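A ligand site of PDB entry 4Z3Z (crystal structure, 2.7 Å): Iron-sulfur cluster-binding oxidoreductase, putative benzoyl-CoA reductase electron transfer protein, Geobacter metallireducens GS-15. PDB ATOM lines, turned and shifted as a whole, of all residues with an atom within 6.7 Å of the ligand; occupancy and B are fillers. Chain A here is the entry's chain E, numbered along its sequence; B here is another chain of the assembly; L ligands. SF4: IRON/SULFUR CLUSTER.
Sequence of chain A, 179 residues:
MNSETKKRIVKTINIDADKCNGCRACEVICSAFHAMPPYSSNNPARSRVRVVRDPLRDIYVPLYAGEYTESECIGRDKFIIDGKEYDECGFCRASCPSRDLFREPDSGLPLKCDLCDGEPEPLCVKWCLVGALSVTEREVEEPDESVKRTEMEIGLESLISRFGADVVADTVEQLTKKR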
ATOM      1  N   ILE A  15      -2.457 -16.848 -18.383  1.00  0.00           N
ATOM      2  CA  ILE A  15      -1.091 -16.899 -18.860  1.00  0.00           C
ATOM      3  C   ILE A  15      -0.276 -15.829 -18.169  1.00  0.00           C
ATOM      4  O   ILE A  15      -0.523 -14.629 -18.328  1.00  0.00           O
ATOM      5  CB  ILE A  15      -1.030 -16.698 -20.390  1.00  0.00           C
ATOM      6  CG1 ILE A  15      -1.903 -17.739 -21.091  1.00  0.00           C
ATOM      7  CG2 ILE A  15       0.406 -16.752 -20.866  1.00  0.00           C
ATOM      8  CD1 ILE A  15      -1.929 -17.614 -22.592  1.00  0.00           C
ATOM      9  N   ASP A  16       0.695 -16.262 -17.364  1.00  0.00           N
ATOM     10  CA  ASP A  16       1.587 -15.355 -16.660  1.00  0.00           C
ATOM     11  C   ASP A  16       2.891 -15.193 -17.433  1.00  0.00           C
ATOM     12  O   ASP A  16       3.853 -15.932 -17.213  1.00  0.00           O
ATOM     13  CB  ASP A  16       1.858 -15.866 -15.236  1.00  0.00           C
ATOM     14  CG  ASP A  16       2.390 -14.783 -14.311  1.00  0.00           C
ATOM     15  OD1 ASP A  16       2.872 -13.736 -14.813  1.00  0.00           O
ATOM     16  OD2 ASP A  16       2.340 -14.971 -13.074  1.00  0.00           O
ATOM     17  N   LYS A  19       6.162 -14.991 -15.647  1.00  0.00           N
ATOM     18  CA  LYS A  19       6.740 -16.175 -15.001  1.00  0.00           C
ATOM     19  C   LYS A  19       7.395 -17.119 -15.999  1.00  0.00           C
ATOM     20  O   LYS A  19       8.261 -17.915 -15.638  1.00  0.00           O
ATOM     21  CB  LYS A  19       5.666 -16.920 -14.204  1.00  0.00           C
ATOM     22  CG  LYS A  19       5.353 -16.303 -12.856  1.00  0.00           C
ATOM     23  CD  LYS A  19       4.396 -17.165 -12.067  1.00  0.00           C
ATOM     24  CE  LYS A  19       4.054 -16.530 -10.729  1.00  0.00           C
ATOM     25  NZ  LYS A  19       3.074 -17.338  -9.950  1.00  0.00           N
ATOM     26  N   CYS A  20       6.956 -17.055 -17.252  1.00  0.00           N
ATOM     27  CA  CYS A  20       7.511 -17.907 -18.297  1.00  0.00           C
ATOM     28  C   CYS A  20       8.990 -17.594 -18.516  1.00  0.00           C
ATOM     29  O   CYS A  20       9.384 -16.432 -18.526  1.00  0.00           O
ATOM     30  CB  CYS A  20       6.735 -17.733 -19.604  1.00  0.00           C
ATOM     31  SG  CYS A  20       7.553 -18.406 -21.048  1.00  0.00           S
ATOM     32  N   ASN A  21       9.803 -18.639 -18.686  1.00  0.00           N
ATOM     33  CA  ASN A  21      11.244 -18.468 -18.815  1.00  0.00           C
ATOM     34  C   ASN A  21      11.759 -18.786 -20.209  1.00  0.00           C
ATOM     35  O   ASN A  21      12.973 -18.874 -20.428  1.00  0.00           O
ATOM     36  CB  ASN A  21      11.972 -19.324 -17.780  1.00  0.00           C
ATOM     37  CG  ASN A  21      11.482 -20.750 -17.786  1.00  0.00           C
ATOM     38  OD1 ASN A  21      11.651 -21.467 -18.765  1.00  0.00           O
ATOM     39  ND2 ASN A  21      10.883 -21.175 -16.673  1.00  0.00           N
ATOM     40  N   GLY A  22      10.839 -18.989 -21.152  1.00  0.00           N
ATOM     41  CA  GLY A  22      11.172 -19.143 -22.551  1.00  0.00           C
ATOM     42  C   GLY A  22      11.546 -20.540 -22.993  1.00  0.00           C
ATOM     43  O   GLY A  22      11.991 -20.728 -24.133  1.00  0.00           O
ATOM     44  N   CYS A  23      11.341 -21.515 -22.109  1.00  0.00           N
ATOM     45  CA  CYS A  23      11.886 -22.868 -22.308  1.00  0.00           C
ATOM     46  C   CYS A  23      11.243 -23.633 -23.455  1.00  0.00           C
ATOM     47  O   CYS A  23      11.827 -24.581 -23.980  1.00  0.00           O
ATOM     48  CB  CYS A  23      11.747 -23.681 -21.022  1.00  0.00           C
ATOM     49  SG  CYS A  23      10.046 -24.158 -20.646  1.00  0.00           S
ATOM     50  N   ARG A  24      10.033 -23.208 -23.833  1.00  0.00           N
ATOM     51  CA  ARG A  24       9.275 -23.823 -24.920  1.00  0.00           C
ATOM     52  C   ARG A  24       8.928 -25.294 -24.677  1.00  0.00           C
ATOM     53  O   ARG A  24       8.725 -26.051 -25.617  1.00  0.00           O
ATOM     54  CB  ARG A  24      10.035 -23.714 -26.248  1.00  0.00           C
ATOM     55  CG  ARG A  24      10.231 -22.301 -26.738  1.00  0.00           C
ATOM     56  CD  ARG A  24      11.110 -22.301 -27.978  1.00  0.00           C
ATOM     57  NE  ARG A  24      10.705 -23.324 -28.927  1.00  0.00           N
ATOM     58  CZ  ARG A  24      11.420 -23.682 -30.001  1.00  0.00           C
ATOM     59  NH1 ARG A  24      12.573 -23.082 -30.247  1.00  0.00           N
ATOM     60  NH2 ARG A  24      10.972 -24.629 -30.810  1.00  0.00           N
ATOM     61  N   ALA A  25       8.852 -25.685 -23.405  1.00  0.00           N
ATOM     62  CA  ALA A  25       8.451 -27.046 -23.049  1.00  0.00           C
ATOM     63  C   ALA A  25       6.970 -27.297 -23.350  1.00  0.00           C
ATOM     64  O   ALA A  25       6.558 -28.422 -23.685  1.00  0.00           O
ATOM     65  CB  ALA A  25       8.751 -27.314 -21.576  1.00  0.00           C
ATOM     66  N   CYS A  26       6.157 -26.249 -23.222  1.00  0.00           N
ATOM     67  CA  CYS A  26       4.755 -26.304 -23.604  1.00  0.00           C
ATOM     68  C   CYS A  26       4.589 -26.779 -25.044  1.00  0.00           C
ATOM     69  O   CYS A  26       3.816 -27.703 -25.308  1.00  0.00           O
ATOM     70  CB  CYS A  26       4.107 -24.943 -23.419  1.00  0.00           C
ATOM     71  SG  CYS A  26       5.260 -23.573 -23.572  1.00  0.00           S
ATOM     72  N   GLU A  27       5.321 -26.159 -25.956  1.00  0.00           N
ATOM     73  CA  GLU A  27       5.313 -26.550 -27.370  1.00  0.00           C
ATOM     74  C   GLU A  27       5.637 -28.036 -27.538  1.00  0.00           C
ATOM     75  O   GLU A  27       4.908 -28.769 -28.220  1.00  0.00           O
ATOM     76  CB  GLU A  27       6.308 -25.708 -28.177  1.00  0.00           C
ATOM     77  CG  GLU A  27       6.002 -24.209 -28.203  1.00  0.00           C
ATOM     78  CD  GLU A  27       7.021 -23.427 -29.031  1.00  0.00           C
ATOM     79  OE1 GLU A  27       8.021 -24.034 -29.460  1.00  0.00           O
ATOM     80  OE2 GLU A  27       6.821 -22.218 -29.249  1.00  0.00           O
ATOM     81  N   VAL A  49      -0.086 -24.285 -28.673  1.00  0.00           N
ATOM     82  CA  VAL A  49       0.502 -23.139 -27.998  1.00  0.00           C
ATOM     83  C   VAL A  49       1.875 -22.846 -28.597  1.00  0.00           C
ATOM     84  O   VAL A  49       2.698 -23.736 -28.784  1.00  0.00           O
ATOM     85  CB  VAL A  49       0.640 -23.367 -26.475  1.00  0.00           C
ATOM     86  CG1 VAL A  49       1.405 -24.658 -26.163  1.00  0.00           C
ATOM     87  CG2 VAL A  49       1.303 -22.157 -25.810  1.00  0.00           C
ATOM     88  N   VAL A  51       5.142 -20.061 -28.223  1.00  0.00           N
ATOM     89  CA  VAL A  51       5.668 -19.017 -27.372  1.00  0.00           C
ATOM     90  C   VAL A  51       6.413 -17.948 -28.169  1.00  0.00           C
ATOM     91  O   VAL A  51       7.439 -18.215 -28.777  1.00  0.00           O
ATOM     92  CB  VAL A  51       6.605 -19.575 -26.286  1.00  0.00           C
ATOM     93  CG1 VAL A  51       7.110 -18.456 -25.404  1.00  0.00           C
ATOM     94  CG2 VAL A  51       5.861 -20.615 -25.459  1.00  0.00           C
ATOM     95  N   TYR A  60       8.612 -12.756 -23.453  1.00  0.00           N
ATOM     96  CA  TYR A  60       8.274 -14.162 -23.348  1.00  0.00           C
ATOM     97  C   TYR A  60       6.756 -14.256 -23.165  1.00  0.00           C
ATOM     98  O   TYR A  60       6.237 -13.946 -22.088  1.00  0.00           O
ATOM     99  CB  TYR A  60       9.036 -14.826 -22.197  1.00  0.00           C
ATOM    100  CG  TYR A  60      10.510 -14.469 -22.125  1.00  0.00           C
ATOM    101  CD1 TYR A  60      10.929 -13.271 -21.549  1.00  0.00           C
ATOM    102  CD2 TYR A  60      11.491 -15.329 -22.619  1.00  0.00           C
ATOM    103  CE1 TYR A  60      12.279 -12.935 -21.485  1.00  0.00           C
ATOM    104  CE2 TYR A  60      12.832 -14.998 -22.558  1.00  0.00           C
ATOM    105  CZ  TYR A  60      13.221 -13.803 -21.992  1.00  0.00           C
ATOM    106  OH  TYR A  60      14.568 -13.467 -21.918  1.00  0.00           O
ATOM    107  N   PRO A  62       3.431 -16.823 -24.044  1.00  0.00           N
ATOM    108  CA  PRO A  62       2.739 -17.982 -24.617  1.00  0.00           C
ATOM    109  C   PRO A  62       1.434 -17.580 -25.298  1.00  0.00           C
ATOM    110  O   PRO A  62       0.599 -16.923 -24.691  1.00  0.00           O
ATOM    111  CB  PRO A  62       2.470 -18.873 -23.390  1.00  0.00           C
ATOM    112  CG  PRO A  62       3.408 -18.375 -22.331  1.00  0.00           C
ATOM    113  CD  PRO A  62       3.581 -16.915 -22.589  1.00  0.00           C
ATOM    114  N   CYS A 124       0.142 -28.823 -21.378  1.00  0.00           N
ATOM    115  CA  CYS A 124       0.988 -27.631 -21.369  1.00  0.00           C
ATOM    116  C   CYS A 124       1.176 -27.095 -19.947  1.00  0.00           C
ATOM    117  O   CYS A 124       2.218 -26.529 -19.616  1.00  0.00           O
ATOM    118  CB  CYS A 124       0.413 -26.544 -22.292  1.00  0.00           C
ATOM    119  SG  CYS A 124      -1.372 -26.210 -22.105  1.00  0.00           S
ATOM    120  N   TRP A 127       3.450 -29.686 -17.603  1.00  0.00           N
ATOM    121  CA  TRP A 127       4.858 -29.608 -17.969  1.00  0.00           C
ATOM    122  C   TRP A 127       5.417 -28.209 -17.801  1.00  0.00           C
ATOM    123  O   TRP A 127       6.456 -27.873 -18.355  1.00  0.00           O
ATOM    124  CB  TRP A 127       5.037 -30.058 -19.412  1.00  0.00           C
ATOM    125  CG  TRP A 127       5.114 -31.524 -19.558  1.00  0.00           C
ATOM    126  CD1 TRP A 127       4.299 -32.446 -18.992  1.00  0.00           C
ATOM    127  CD2 TRP A 127       6.068 -32.251 -20.332  1.00  0.00           C
ATOM    128  NE1 TRP A 127       4.678 -33.706 -19.366  1.00  0.00           N
ATOM    129  CE2 TRP A 127       5.774 -33.608 -20.183  1.00  0.00           C
ATOM    130  CE3 TRP A 127       7.153 -31.879 -21.136  1.00  0.00           C
ATOM    131  CZ2 TRP A 127       6.521 -34.616 -20.809  1.00  0.00           C
ATOM    132  CZ3 TRP A 127       7.889 -32.868 -21.756  1.00  0.00           C
ATOM    133  CH2 TRP A 127       7.576 -34.219 -21.593  1.00  0.00           C
ATOM    134  N   CYS A 128       4.713 -27.376 -17.035  1.00  0.00           N
ATOM    135  CA  CYS A 128       5.187 -26.036 -16.756  1.00  0.00           C
ATOM    136  C   CYS A 128       5.509 -25.928 -15.276  1.00  0.00           C
ATOM    137  O   CYS A 128       4.783 -25.314 -14.505  1.00  0.00           O
ATOM    138  CB  CYS A 128       4.149 -24.993 -17.175  1.00  0.00           C
ATOM    139  SG  CYS A 128       4.787 -23.298 -17.251  1.00  0.00           S
ATOM    140  N   LEU A 129       6.612 -26.563 -14.890  1.00  0.00           N
ATOM    141  CA  LEU A 129       7.016 -26.692 -13.497  1.00  0.00           C
ATOM    142  C   LEU A 129       7.188 -25.335 -12.811  1.00  0.00           C
ATOM    143  O   LEU A 129       7.097 -25.243 -11.582  1.00  0.00           O
ATOM    144  CB  LEU A 129       8.312 -27.499 -13.396  1.00  0.00           C
ATOM    145  CG  LEU A 129       8.231 -29.023 -13.495  1.00  0.00           C
ATOM    146  CD1 LEU A 129       7.656 -29.508 -14.825  1.00  0.00           C
ATOM    147  CD2 LEU A 129       9.611 -29.636 -13.262  1.00  0.00           C
ATOM    148  N   VAL A 130       7.424 -24.308 -13.614  1.00  0.00           N
ATOM    149  CA  VAL A 130       7.604 -22.942 -13.126  1.00  0.00           C
ATOM    150  C   VAL A 130       6.234 -22.323 -12.787  1.00  0.00           C
ATOM    151  O   VAL A 130       6.151 -21.296 -12.103  1.00  0.00           O
ATOM    152  CB  VAL A 130       8.372 -22.086 -14.156  1.00  0.00           C
ATOM    153  CG1 VAL A 130       7.570 -21.927 -15.428  1.00  0.00           C
ATOM    154  CG2 VAL A 130       8.754 -20.725 -13.570  1.00  0.00           C
ATOM    155  N   GLY A 131       5.174 -22.957 -13.256  1.00  0.00           N
ATOM    156  CA  GLY A 131       3.824 -22.515 -12.964  1.00  0.00           C
ATOM    157  C   GLY A 131       3.432 -21.195 -13.609  1.00  0.00           C
ATOM    158  O   GLY A 131       3.169 -20.209 -12.908  1.00  0.00           O
ATOM    159  N   ALA A 132       3.388 -21.165 -14.932  1.00  0.00           N
ATOM    160  CA  ALA A 132       3.063 -19.940 -15.644  1.00  0.00           C
ATOM    161  C   ALA A 132       1.734 -20.045 -16.379  1.00  0.00           C
ATOM    162  O   ALA A 132       1.238 -19.062 -16.934  1.00  0.00           O
ATOM    163  CB  ALA A 132       4.178 -19.590 -16.627  1.00  0.00           C
ATOM    164  N   LEU A 133       1.137 -21.238 -16.370  1.00  0.00           N
ATOM    165  CA  LEU A 133      -0.114 -21.479 -17.071  1.00  0.00           C
ATOM    166  C   LEU A 133      -1.166 -22.104 -16.158  1.00  0.00           C
ATOM    167  O   LEU A 133      -0.968 -23.202 -15.652  1.00  0.00           O
ATOM    168  CB  LEU A 133       0.123 -22.387 -18.270  1.00  0.00           C
ATOM    169  CG  LEU A 133       1.282 -22.064 -19.205  1.00  0.00           C
ATOM    170  CD1 LEU A 133       1.470 -23.168 -20.230  1.00  0.00           C
ATOM    171  CD2 LEU A 133       1.059 -20.726 -19.901  1.00  0.00           C
ATOM    172  N   SER B 298      15.855 -20.249 -19.356  1.00  0.00           N
ATOM    173  CA  SER B 298      16.216 -21.652 -19.517  1.00  0.00           C
ATOM    174  C   SER B 298      16.722 -21.997 -20.912  1.00  0.00           C
ATOM    175  O   SER B 298      16.583 -21.224 -21.855  1.00  0.00           O
ATOM    176  CB  SER B 298      15.009 -22.542 -19.229  1.00  0.00           C
ATOM    177  OG  SER B 298      14.606 -22.450 -17.881  1.00  0.00           O
ATOM    178  N   CYS B 302      13.454 -27.105 -20.281  1.00  0.00           N
ATOM    179  CA  CYS B 302      14.006 -27.245 -18.934  1.00  0.00           C
ATOM    180  C   CYS B 302      13.489 -26.144 -17.996  1.00  0.00           C
ATOM    181  O   CYS B 302      13.400 -24.988 -18.385  1.00  0.00           O
ATOM    182  CB  CYS B 302      15.544 -27.205 -18.981  1.00  0.00           C
ATOM    183  SG  CYS B 302      16.343 -27.444 -17.379  1.00  0.00           S
HETATM  184 FE1  SF4 L   1       5.489 -22.718 -21.459  1.00  0.00          FE
HETATM  185 FE2  SF4 L   1       6.207 -22.471 -18.835  1.00  0.00          FE
HETATM  186 FE3  SF4 L   1       6.719 -20.512 -20.612  1.00  0.00          FE
HETATM  187 FE4  SF4 L   1       8.090 -22.928 -20.649  1.00  0.00          FE
HETATM  188  S1  SF4 L   1       8.186 -21.317 -19.012  1.00  0.00           S
HETATM  189  S2  SF4 L   1       7.313 -21.758 -22.454  1.00  0.00           S
HETATM  190  S3  SF4 L   1       6.367 -24.370 -20.130  1.00  0.00           S
HETATM  191  S4  SF4 L   1       4.652 -21.190 -19.954  1.00  0.00           S
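An iron atom (FE2) of the ligand is bound by the side-chain sulfur of Cys 128 (2.3 Å). The backbone NH of Cys 26 sits close to a sulfur (S3) of the ligand, 3.6 Å away. FE1 of the ligand is bound by SG of Cys 26. SG of Cys 20 binds FE3 of the ligand (2.3 Å). SG of Cys 23 binds FE4 of the ligand. The backbone NH (N) of Asn 21 sits close to a sulfur (S1) of the ligand (3.1 Å). S1 of the ligand lies close to OD1 of Asn 21 (3.5 Å). A sulfur (S2) of the ligand lies close to the backbone NH (N) of Arg 24, 3.4 Å away.
Residues that only touch the ligand: Val 51 (3.5 Å), Leu 133 (3.6 Å), Val 130 (3.7 Å), Ala 132 (3.7 Å), Pro 62 (3.9 Å), Trp 127 (3.9 Å) and Ala 25 (3.97 Å). Hydrophobic or aromatic side chains that line the ligand: Val 51, Pro 62, Val 130, Ala 132 and Leu 133.
The side-chain sulfur (SG) of Cys 128 lies close to the backbone NH (N) of Ala 132, at 3.4 Å. The side-chain sulfur of Cys 20 lies close to the backbone NH of Gly 22 (3.3 Å). OD1 of Asn 21 sits close to N of Cys 23, at 3.4 Å. SG of Cys 23 lies close to N of Ala 25, at 3.4 Å. The side-chain hydroxyl (OG) of Ser 298 of chain B is in hydrogen-bond range of the side-chain amide oxygen (OD1) of Asn 21. The side-chain carboxylate (OE1) of Glu 27 is in salt-bridge range of the guanidinium group (NE) of Arg 24. The backbone NH of Val 51 sits at hydrogen-bond distance from the side-chain carboxylate of Glu 27 (2.9 Å). O of Ala 132 sits at hydrogen-bond distance from N of Asp 16.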
